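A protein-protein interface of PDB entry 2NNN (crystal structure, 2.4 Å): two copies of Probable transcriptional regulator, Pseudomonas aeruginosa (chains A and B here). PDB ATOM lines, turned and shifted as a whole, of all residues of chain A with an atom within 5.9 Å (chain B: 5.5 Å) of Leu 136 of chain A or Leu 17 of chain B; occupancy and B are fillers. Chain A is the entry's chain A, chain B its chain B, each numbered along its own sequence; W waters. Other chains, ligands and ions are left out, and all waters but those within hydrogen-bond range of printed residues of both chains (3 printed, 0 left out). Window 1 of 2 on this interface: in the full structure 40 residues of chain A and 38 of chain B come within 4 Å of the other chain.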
ATOM      1  N   LEU A  17     -20.126  -4.553  -4.875  1.00  0.00           N
ATOM      2  CA  LEU A  17     -18.978  -3.982  -4.149  1.00  0.00           C
ATOM      3  C   LEU A  17     -19.130  -2.502  -3.884  1.00  0.00           C
ATOM      4  O   LEU A  17     -18.855  -2.054  -2.787  1.00  0.00           O
ATOM      5  CB  LEU A  17     -17.661  -4.241  -4.881  1.00  0.00           C
ATOM      6  CG  LEU A  17     -17.128  -5.661  -4.825  1.00  0.00           C
ATOM      7  CD1 LEU A  17     -15.894  -5.772  -5.735  1.00  0.00           C
ATOM      8  CD2 LEU A  17     -16.831  -6.042  -3.387  1.00  0.00           C
ATOM      9  N   ALA A  20     -21.924  -1.954  -1.072  1.00  0.00           N
ATOM     10  CA  ALA A  20     -21.328  -2.311   0.226  1.00  0.00           C
ATOM     11  C   ALA A  20     -20.354  -1.217   0.685  1.00  0.00           C
ATOM     12  O   ALA A  20     -20.331  -0.831   1.861  1.00  0.00           O
ATOM     13  CB  ALA A  20     -20.623  -3.647   0.124  1.00  0.00           C
ATOM     14  N   ASN A  21     -19.565  -0.713  -0.259  1.00  0.00           N
ATOM     15  CA  ASN A  21     -18.662   0.398  -0.012  1.00  0.00           C
ATOM     16  C   ASN A  21     -19.410   1.664   0.412  1.00  0.00           C
ATOM     17  O   ASN A  21     -19.037   2.288   1.401  1.00  0.00           O
ATOM     18  CB  ASN A  21     -17.796   0.652  -1.246  1.00  0.00           C
ATOM     19  CG  ASN A  21     -16.343   0.940  -0.906  1.00  0.00           C
ATOM     20  OD1 ASN A  21     -15.812   1.980  -1.293  1.00  0.00           O
ATOM     21  ND2 ASN A  21     -15.686   0.031  -0.216  1.00  0.00           N
ATOM     22  N   TYR A  24     -20.848   1.276   3.923  1.00  0.00           N
ATOM     23  CA  TYR A  24     -19.772   1.405   4.893  1.00  0.00           C
ATOM     24  C   TYR A  24     -19.443   2.875   5.109  1.00  0.00           C
ATOM     25  O   TYR A  24     -19.334   3.334   6.251  1.00  0.00           O
ATOM     26  CB  TYR A  24     -18.519   0.592   4.498  1.00  0.00           C
ATOM     27  CG  TYR A  24     -17.486   0.684   5.585  1.00  0.00           C
ATOM     28  CD1 TYR A  24     -17.519  -0.195   6.674  1.00  0.00           C
ATOM     29  CD2 TYR A  24     -16.512   1.698   5.573  1.00  0.00           C
ATOM     30  CE1 TYR A  24     -16.601  -0.091   7.698  1.00  0.00           C
ATOM     31  CE2 TYR A  24     -15.593   1.806   6.596  1.00  0.00           C
ATOM     32  CZ  TYR A  24     -15.652   0.905   7.656  1.00  0.00           C
ATOM     33  OH  TYR A  24     -14.750   1.005   8.684  1.00  0.00           O
ATOM     34  N   THR A 131     -16.346 -16.342   7.199  1.00  0.00           N
ATOM     35  CA  THR A 131     -16.406 -16.825   5.825  1.00  0.00           C
ATOM     36  C   THR A 131     -16.266 -15.661   4.846  1.00  0.00           C
ATOM     37  O   THR A 131     -15.491 -15.732   3.900  1.00  0.00           O
ATOM     38  CB  THR A 131     -17.739 -17.545   5.540  1.00  0.00           C
ATOM     39  OG1 THR A 131     -17.923 -18.602   6.484  1.00  0.00           O
ATOM     40  CG2 THR A 131     -17.769 -18.109   4.121  1.00  0.00           C
ATOM     41  N   LEU A 132     -17.019 -14.592   5.081  1.00  0.00           N
ATOM     42  CA  LEU A 132     -17.004 -13.436   4.189  1.00  0.00           C
ATOM     43  C   LEU A 132     -15.636 -12.762   4.157  1.00  0.00           C
ATOM     44  O   LEU A 132     -15.114 -12.497   3.090  1.00  0.00           O
ATOM     45  CB  LEU A 132     -18.096 -12.421   4.562  1.00  0.00           C
ATOM     46  CG  LEU A 132     -18.020 -11.112   3.774  1.00  0.00           C
ATOM     47  CD1 LEU A 132     -18.675 -11.225   2.390  1.00  0.00           C
ATOM     48  CD2 LEU A 132     -18.625  -9.995   4.573  1.00  0.00           C
ATOM     49  N   ARG A 133     -15.063 -12.502   5.327  1.00  0.00           N
ATOM     50  CA  ARG A 133     -13.742 -11.883   5.418  1.00  0.00           C
ATOM     51  C   ARG A 133     -12.687 -12.691   4.642  1.00  0.00           C
ATOM     52  O   ARG A 133     -11.856 -12.102   3.939  1.00  0.00           O
ATOM     53  CB  ARG A 133     -13.331 -11.713   6.890  1.00  0.00           C
ATOM     54  CG  ARG A 133     -12.524 -10.438   7.194  1.00  0.00           C
ATOM     55  CD  ARG A 133     -12.198 -10.270   8.698  1.00  0.00           C
ATOM     56  NE  ARG A 133     -13.309 -10.675   9.569  1.00  0.00           N
ATOM     57  CZ  ARG A 133     -14.016  -9.850  10.342  1.00  0.00           C
ATOM     58  NH1 ARG A 133     -13.743  -8.544  10.387  1.00  0.00           N
ATOM     59  NH2 ARG A 133     -15.000 -10.339  11.084  1.00  0.00           N
ATOM     60  N   GLY A 134     -12.744 -14.024   4.761  1.00  0.00           N
ATOM     61  CA  GLY A 134     -11.838 -14.937   4.058  1.00  0.00           C
ATOM     62  C   GLY A 134     -12.002 -14.930   2.546  1.00  0.00           C
ATOM     63  O   GLY A 134     -11.024 -14.805   1.802  1.00  0.00           O
ATOM     64  N   LEU A 135     -13.246 -15.075   2.095  1.00  0.00           N
ATOM     65  CA  LEU A 135     -13.601 -14.973   0.679  1.00  0.00           C
ATOM     66  C   LEU A 135     -13.242 -13.601   0.086  1.00  0.00           C
ATOM     67  O   LEU A 135     -12.648 -13.518  -0.985  1.00  0.00           O
ATOM     68  CB  LEU A 135     -15.095 -15.274   0.500  1.00  0.00           C
ATOM     69  CG  LEU A 135     -15.591 -16.695   0.178  1.00  0.00           C
ATOM     70  CD1 LEU A 135     -14.755 -17.817   0.806  1.00  0.00           C
ATOM     71  CD2 LEU A 135     -17.065 -16.846   0.537  1.00  0.00           C
ATOM     72  N   LEU A 136     -13.583 -12.533   0.797  1.00  0.00           N
ATOM     73  CA  LEU A 136     -13.319 -11.167   0.346  1.00  0.00           C
ATOM     74  C   LEU A 136     -11.817 -10.801   0.386  1.00  0.00           C
ATOM     75  O   LEU A 136     -11.347 -10.004  -0.427  1.00  0.00           O
ATOM     76  CB  LEU A 136     -14.167 -10.179   1.161  1.00  0.00           C
ATOM     77  CG  LEU A 136     -14.650  -8.844   0.571  1.00  0.00           C
ATOM     78  CD1 LEU A 136     -15.446  -9.006  -0.735  1.00  0.00           C
ATOM     79  CD2 LEU A 136     -15.461  -8.061   1.591  1.00  0.00           C
ATOM     80  N   ALA A 137     -11.060 -11.396   1.308  1.00  0.00           N
ATOM     81  CA  ALA A 137      -9.601 -11.182   1.371  1.00  0.00           C
ATOM     82  C   ALA A 137      -8.904 -11.638   0.094  1.00  0.00           C
ATOM     83  O   ALA A 137      -7.875 -11.074  -0.314  1.00  0.00           O
ATOM     84  CB  ALA A 137      -9.007 -11.906   2.566  1.00  0.00           C
ATOM     85  N   ARG A 138      -9.476 -12.672  -0.522  1.00  0.00           N
ATOM     86  CA  ARG A 138      -8.980 -13.250  -1.752  1.00  0.00           C
ATOM     87  C   ARG A 138      -9.346 -12.411  -2.983  1.00  0.00           C
ATOM     88  O   ARG A 138      -8.900 -12.719  -4.093  1.00  0.00           O
ATOM     89  CB  ARG A 138      -9.522 -14.682  -1.894  1.00  0.00           C
ATOM     90  CG  ARG A 138      -8.937 -15.684  -0.864  1.00  0.00           C
ATOM     91  CD  ARG A 138      -9.802 -16.944  -0.699  1.00  0.00           C
ATOM     92  NE  ARG A 138      -9.884 -17.718  -1.936  1.00  0.00           N
ATOM     93  CZ  ARG A 138     -10.642 -18.798  -2.104  1.00  0.00           C
ATOM     94  NH1 ARG A 138     -11.387 -19.253  -1.102  1.00  0.00           N
ATOM     95  NH2 ARG A 138     -10.646 -19.430  -3.277  1.00  0.00           N
ATOM     96  N   LEU A 139     -10.156 -11.363  -2.787  1.00  0.00           N
ATOM     97  CA  LEU A 139     -10.579 -10.476  -3.880  1.00  0.00           C
ATOM     98  C   LEU A 139      -9.968  -9.079  -3.779  1.00  0.00           C
ATOM     99  O   LEU A 139     -10.296  -8.180  -4.557  1.00  0.00           O
ATOM    100  CB  LEU A 139     -12.109 -10.365  -3.937  1.00  0.00           C
ATOM    101  CG  LEU A 139     -12.939 -11.610  -4.276  1.00  0.00           C
ATOM    102  CD1 LEU A 139     -14.304 -11.157  -4.769  1.00  0.00           C
ATOM    103  CD2 LEU A 139     -12.252 -12.503  -5.314  1.00  0.00           C
ATOM    104  N   ILE A 140      -9.082  -8.915  -2.805  1.00  0.00           N
ATOM    105  CA  ILE A 140      -8.376  -7.667  -2.544  1.00  0.00           C
ATOM    106  C   ILE A 140      -7.382  -7.360  -3.656  1.00  0.00           C
ATOM    107  O   ILE A 140      -7.082  -6.210  -3.965  1.00  0.00           O
ATOM    108  CB  ILE A 140      -7.752  -7.720  -1.110  1.00  0.00           C
ATOM    109  CG1 ILE A 140      -8.532  -6.808  -0.176  1.00  0.00           C
ATOM    110  CG2 ILE A 140      -6.246  -7.418  -1.068  1.00  0.00           C
ATOM    111  CD1 ILE A 140      -9.998  -7.092  -0.181  1.00  0.00           C
ATOM    112  OXT ILE A 140      -6.875  -8.267  -4.296  1.00  0.00           O
ATOM    113  N   GLN B  12     -10.120  -4.853   9.100  1.00  0.00           N
ATOM    114  CA  GLN B  12     -11.301  -4.001   9.052  1.00  0.00           C
ATOM    115  C   GLN B  12     -11.992  -4.169   7.720  1.00  0.00           C
ATOM    116  O   GLN B  12     -11.373  -4.020   6.666  1.00  0.00           O
ATOM    117  CB  GLN B  12     -10.930  -2.535   9.311  1.00  0.00           C
ATOM    118  CG  GLN B  12     -10.196  -2.337  10.630  1.00  0.00           C
ATOM    119  CD  GLN B  12     -10.965  -2.919  11.808  1.00  0.00           C
ATOM    120  OE1 GLN B  12     -12.126  -2.549  12.054  1.00  0.00           O
ATOM    121  NE2 GLN B  12     -10.328  -3.840  12.538  1.00  0.00           N
ATOM    122  N   ILE B  13     -13.282  -4.484   7.772  1.00  0.00           N
ATOM    123  CA  ILE B  13     -14.047  -4.749   6.567  1.00  0.00           C
ATOM    124  C   ILE B  13     -14.089  -3.525   5.642  1.00  0.00           C
ATOM    125  O   ILE B  13     -14.167  -3.665   4.425  1.00  0.00           O
ATOM    126  CB  ILE B  13     -15.449  -5.318   6.890  1.00  0.00           C
ATOM    127  CG1 ILE B  13     -16.103  -5.927   5.639  1.00  0.00           C
ATOM    128  CG2 ILE B  13     -16.344  -4.251   7.523  1.00  0.00           C
ATOM    129  CD1 ILE B  13     -15.492  -7.224   5.177  1.00  0.00           C
ATOM    130  N   GLY B  14     -13.997  -2.331   6.213  1.00  0.00           N
ATOM    131  CA  GLY B  14     -13.926  -1.105   5.414  1.00  0.00           C
ATOM    132  C   GLY B  14     -12.715  -1.028   4.502  1.00  0.00           C
ATOM    133  O   GLY B  14     -12.843  -0.664   3.353  1.00  0.00           O
ATOM    134  N   PHE B  15     -11.543  -1.364   5.029  1.00  0.00           N
ATOM    135  CA  PHE B  15     -10.298  -1.418   4.257  1.00  0.00           C
ATOM    136  C   PHE B  15     -10.407  -2.477   3.157  1.00  0.00           C
ATOM    137  O   PHE B  15     -10.115  -2.206   1.990  1.00  0.00           O
ATOM    138  CB  PHE B  15      -9.126  -1.717   5.210  1.00  0.00           C
ATOM    139  CG  PHE B  15      -7.756  -1.605   4.576  1.00  0.00           C
ATOM    140  CD1 PHE B  15      -7.475  -0.616   3.621  1.00  0.00           C
ATOM    141  CD2 PHE B  15      -6.733  -2.466   4.967  1.00  0.00           C
ATOM    142  CE1 PHE B  15      -6.216  -0.514   3.047  1.00  0.00           C
ATOM    143  CE2 PHE B  15      -5.457  -2.364   4.400  1.00  0.00           C
ATOM    144  CZ  PHE B  15      -5.197  -1.388   3.438  1.00  0.00           C
ATOM    145  N   ILE B  16     -10.846  -3.676   3.548  1.00  0.00           N
ATOM    146  CA  ILE B  16     -11.086  -4.791   2.635  1.00  0.00           C
ATOM    147  C   ILE B  16     -12.049  -4.405   1.505  1.00  0.00           C
ATOM    148  O   ILE B  16     -11.761  -4.643   0.335  1.00  0.00           O
ATOM    149  CB  ILE B  16     -11.576  -6.054   3.421  1.00  0.00           C
ATOM    150  CG1 ILE B  16     -10.495  -6.542   4.423  1.00  0.00           C
ATOM    151  CG2 ILE B  16     -11.937  -7.183   2.487  1.00  0.00           C
ATOM    152  CD1 ILE B  16     -10.983  -7.592   5.420  1.00  0.00           C
ATOM    153  N   LEU B  17     -13.173  -3.778   1.843  1.00  0.00           N
ATOM    154  CA  LEU B  17     -14.125  -3.327   0.809  1.00  0.00           C
ATOM    155  C   LEU B  17     -13.528  -2.348  -0.179  1.00  0.00           C
ATOM    156  O   LEU B  17     -13.739  -2.486  -1.382  1.00  0.00           O
ATOM    157  CB  LEU B  17     -15.413  -2.759   1.408  1.00  0.00           C
ATOM    158  CG  LEU B  17     -16.342  -3.809   2.002  1.00  0.00           C
ATOM    159  CD1 LEU B  17     -17.435  -3.115   2.795  1.00  0.00           C
ATOM    160  CD2 LEU B  17     -16.904  -4.726   0.912  1.00  0.00           C
ATOM    161  N   ARG B  18     -12.758  -1.389   0.319  1.00  0.00           N
ATOM    162  CA  ARG B  18     -12.120  -0.394  -0.553  1.00  0.00           C
ATOM    163  C   ARG B  18     -11.136  -1.015  -1.533  1.00  0.00           C
ATOM    164  O   ARG B  18     -11.082  -0.605  -2.695  1.00  0.00           O
ATOM    165  CB  ARG B  18     -11.420   0.711   0.253  1.00  0.00           C
ATOM    166  CG  ARG B  18     -10.731   1.687  -0.670  1.00  0.00           C
ATOM    167  CD  ARG B  18     -10.368   2.999  -0.029  1.00  0.00           C
ATOM    168  NE  ARG B  18      -9.456   2.894   1.117  1.00  0.00           N
ATOM    169  CZ  ARG B  18      -8.139   2.715   1.042  1.00  0.00           C
ATOM    170  NH1 ARG B  18      -7.545   2.588  -0.135  1.00  0.00           N
ATOM    171  NH2 ARG B  18      -7.415   2.681   2.157  1.00  0.00           N
ATOM    172  N   GLN B  19     -10.360  -1.993  -1.064  1.00  0.00           N
ATOM    173  CA  GLN B  19      -9.345  -2.658  -1.904  1.00  0.00           C
ATOM    174  C   GLN B  19      -9.957  -3.556  -2.975  1.00  0.00           C
ATOM    175  O   GLN B  19      -9.469  -3.603  -4.087  1.00  0.00           O
ATOM    176  CB  GLN B  19      -8.415  -3.499  -1.046  1.00  0.00           C
ATOM    177  CG  GLN B  19      -7.505  -2.718  -0.127  1.00  0.00           C
ATOM    178  CD  GLN B  19      -6.671  -3.652   0.696  1.00  0.00           C
ATOM    179  OE1 GLN B  19      -7.098  -4.149   1.724  1.00  0.00           O
ATOM    180  NE2 GLN B  19      -5.493  -3.917   0.236  1.00  0.00           N
ATOM    181  N   ALA B  20     -10.999  -4.305  -2.610  1.00  0.00           N
ATOM    182  CA  ALA B  20     -11.775  -5.126  -3.559  1.00  0.00           C
ATOM    183  C   ALA B  20     -12.366  -4.221  -4.627  1.00  0.00           C
ATOM    184  O   ALA B  20     -12.317  -4.532  -5.815  1.00  0.00           O
ATOM    185  CB  ALA B  20     -12.874  -5.890  -2.828  1.00  0.00           C
ATOM    186  N   ASN B  21     -12.899  -3.086  -4.191  1.00  0.00           N
ATOM    187  CA  ASN B  21     -13.422  -2.053  -5.072  1.00  0.00           C
ATOM    188  C   ASN B  21     -12.371  -1.438  -6.018  1.00  0.00           C
ATOM    189  O   ASN B  21     -12.650  -1.233  -7.205  1.00  0.00           O
ATOM    190  CB  ASN B  21     -14.065  -0.963  -4.215  1.00  0.00           C
ATOM    191  CG  ASN B  21     -15.348  -0.426  -4.803  1.00  0.00           C
ATOM    192  OD1 ASN B  21     -15.429   0.759  -5.114  1.00  0.00           O
ATOM    193  ND2 ASN B  21     -16.357  -1.265  -4.946  1.00  0.00           N
ATOM    194  N   GLN B  22     -11.179  -1.138  -5.507  1.00  0.00           N
ATOM    195  CA  GLN B  22     -10.088  -0.592  -6.341  1.00  0.00           C
ATOM    196  C   GLN B  22      -9.609  -1.603  -7.374  1.00  0.00           C
ATOM    197  O   GLN B  22      -9.315  -1.226  -8.514  1.00  0.00           O
ATOM    198  CB  GLN B  22      -8.893  -0.136  -5.497  1.00  0.00           C
ATOM    199  CG  GLN B  22      -9.085   1.196  -4.772  1.00  0.00           C
ATOM    200  CD  GLN B  22      -7.938   1.532  -3.818  1.00  0.00           C
ATOM    201  OE1 GLN B  22      -6.850   0.935  -3.869  1.00  0.00           O
ATOM    202  NE2 GLN B  22      -8.179   2.489  -2.944  1.00  0.00           N
ATOM    203  N   LEU B 132     -20.231 -16.039  -1.636  1.00  0.00           N
ATOM    204  CA  LEU B 132     -19.806 -14.647  -1.502  1.00  0.00           C
ATOM    205  C   LEU B 132     -20.861 -13.666  -2.018  1.00  0.00           C
ATOM    206  O   LEU B 132     -21.151 -12.671  -1.369  1.00  0.00           O
ATOM    207  CB  LEU B 132     -18.455 -14.399  -2.187  1.00  0.00           C
ATOM    208  CG  LEU B 132     -18.045 -12.925  -2.238  1.00  0.00           C
ATOM    209  CD1 LEU B 132     -17.349 -12.459  -0.951  1.00  0.00           C
ATOM    210  CD2 LEU B 132     -17.195 -12.662  -3.450  1.00  0.00           C
ATOM    211  N   LEU B 136     -22.417 -11.021   0.517  1.00  0.00           N
ATOM    212  CA  LEU B 136     -22.243  -9.610   0.169  1.00  0.00           C
ATOM    213  C   LEU B 136     -23.569  -8.888  -0.082  1.00  0.00           C
ATOM    214  O   LEU B 136     -23.738  -7.732   0.322  1.00  0.00           O
ATOM    215  CB  LEU B 136     -21.330  -9.454  -1.050  1.00  0.00           C
ATOM    216  CG  LEU B 136     -19.893  -8.939  -0.934  1.00  0.00           C
ATOM    217  CD1 LEU B 136     -19.382  -8.564  -2.327  1.00  0.00           C
ATOM    218  CD2 LEU B 136     -19.744  -7.738   0.018  1.00  0.00           C
HETATM  219  O   HOH W   1     -12.106  -7.284  -6.416  1.00  0.00           O
HETATM  220  O   HOH W   2     -14.606   1.292   2.253  1.00  0.00           O
HETATM  221  O   HOH W   3     -14.209  -1.486   9.274  1.00  0.00           O
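Water W3 lies within hydrogen-bond range of OH of Tyr 24 of chain A (2.6 Å), N of Gly 14 of chain B (3.2 Å) and N of Ile 13 of chain B (3.5 Å). Water W1 lies within hydrogen-bond range of the backbone carbonyl oxygen of Leu 139 of chain A and the backbone carbonyl oxygen of Ala 20 of chain B. Water W2 lies within hydrogen-bond range of the backbone carbonyl oxygen (O) of Gly 14 of chain B (2.9 Å) and the side-chain amide nitrogen (ND2) of Asn 21 of chain A (3.0 Å).
ND2 of Asn 21 of chain A lies close to N of Arg 18 of chain B (3.3 Å). O of Leu 17 of chain B lies close to ND2 of Asn 21 of chain A (3.4 Å). The backbone carbonyl oxygen (O) of Leu 17 of chain A lies close to the side-chain amide nitrogen (ND2) of Asn 21 of chain B (3.4 Å).
Printed residues of chain B within 4 Å of Tyr 24 of chain A: Gly 14. Of the printed residues of chain B, Leu 132 of chain A touches Leu 132 (3.8 Å). Of the printed residues of chain B, Leu 135 of chain A touches Leu 132. Of chain B, only Ile 13, Ile 16, Leu 17 and Leu 132 come within 4 Å of Leu 136 of chain A. Printed residues of chain B within 4 Å of Ile 140 of chain A: Ile 16 (3.1 Å), Gln 19 (3.4 Å) and Ala 20 (3.8 Å). Of chain A, only Ala 20, Asn 21 and Leu 136 come within 4 Å of Leu 17 of chain B. Printed residues of chain A within 4 Å of Arg 18 of chain B: Asn 21. The nearest residue of chain A that does not touch Leu 17 of chain B is Tyr 24 of chain A (4.2 Å). The nearest printed residue of chain B that does not touch Leu 139 of chain A is Gln 19 of chain B (4.7 Å).
Along chain A the printed residues that touch a printed residue of chain B span positions 17 to 140. Hydrophobic or aromatic side chains of chain B within 4 Å of the printed part of chain A: Ile 13, Ile 16, Leu 17, Ala 20, Leu 132 and Leu 136. Among the printed residues, no Asp or Glu carboxylate lies within 4 Å of a Lys or Arg side-chain nitrogen of the other chain.
Among the printed residues, merely in contact across the chains: Leu 17 of chain A with Ala 20 of chain B, Leu 17 of chain A with Leu 136 of chain B, Ala 20 of chain A with Leu 17 of chain B, Tyr 24 of chain A with Gly 14 of chain B, Leu 132 of chain A with Leu 132 of chain B, Arg 133 of chain A with Ile 16 of chain B, Leu 135 of chain A with Leu 132 of chain B, Leu 136 of chain A with Ile 13 of chain B, Leu 136 of chain A with Ile 16 of chain B, Leu 136 of chain A with Leu 17 of chain B, Leu 136 of chain A with Leu 132 of chain B, Leu 139 of chain A with Ala 20 of chain B, Leu 139 of chain A with Leu 132 of chain B, Ile 140 of chain A with Ile 16 of chain B, Ile 140 of chain A with Gln 19 of chain B and Ile 140 of chain A with Ala 20 of chain B.
Leu 17 of chain A touches Ala 20 of chain B, and with the chains exchanged Ala 20 of chain A touches Leu 17 of chain B. Leu 17 of chain A touches Leu 136 of chain B, and with the chains exchanged Leu 136 of chain A touches Leu 17 of chain B. Leu 132 of chain A touches its own counterpart, Leu 132 of chain B. Leu 136 of chain A touches Leu 132 of chain B, but with the chains exchanged Leu 132 of chain A does not touch Leu 136 of chain B (4.2 Å). Of the 19 pairs that touch across the chains among the printed residues, 7 have their exchanged pair printed and touching as well.
NH1 of Arg 18 of chain B lies close to NE2 of Gln 22 of chain B, 2.9 Å away.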
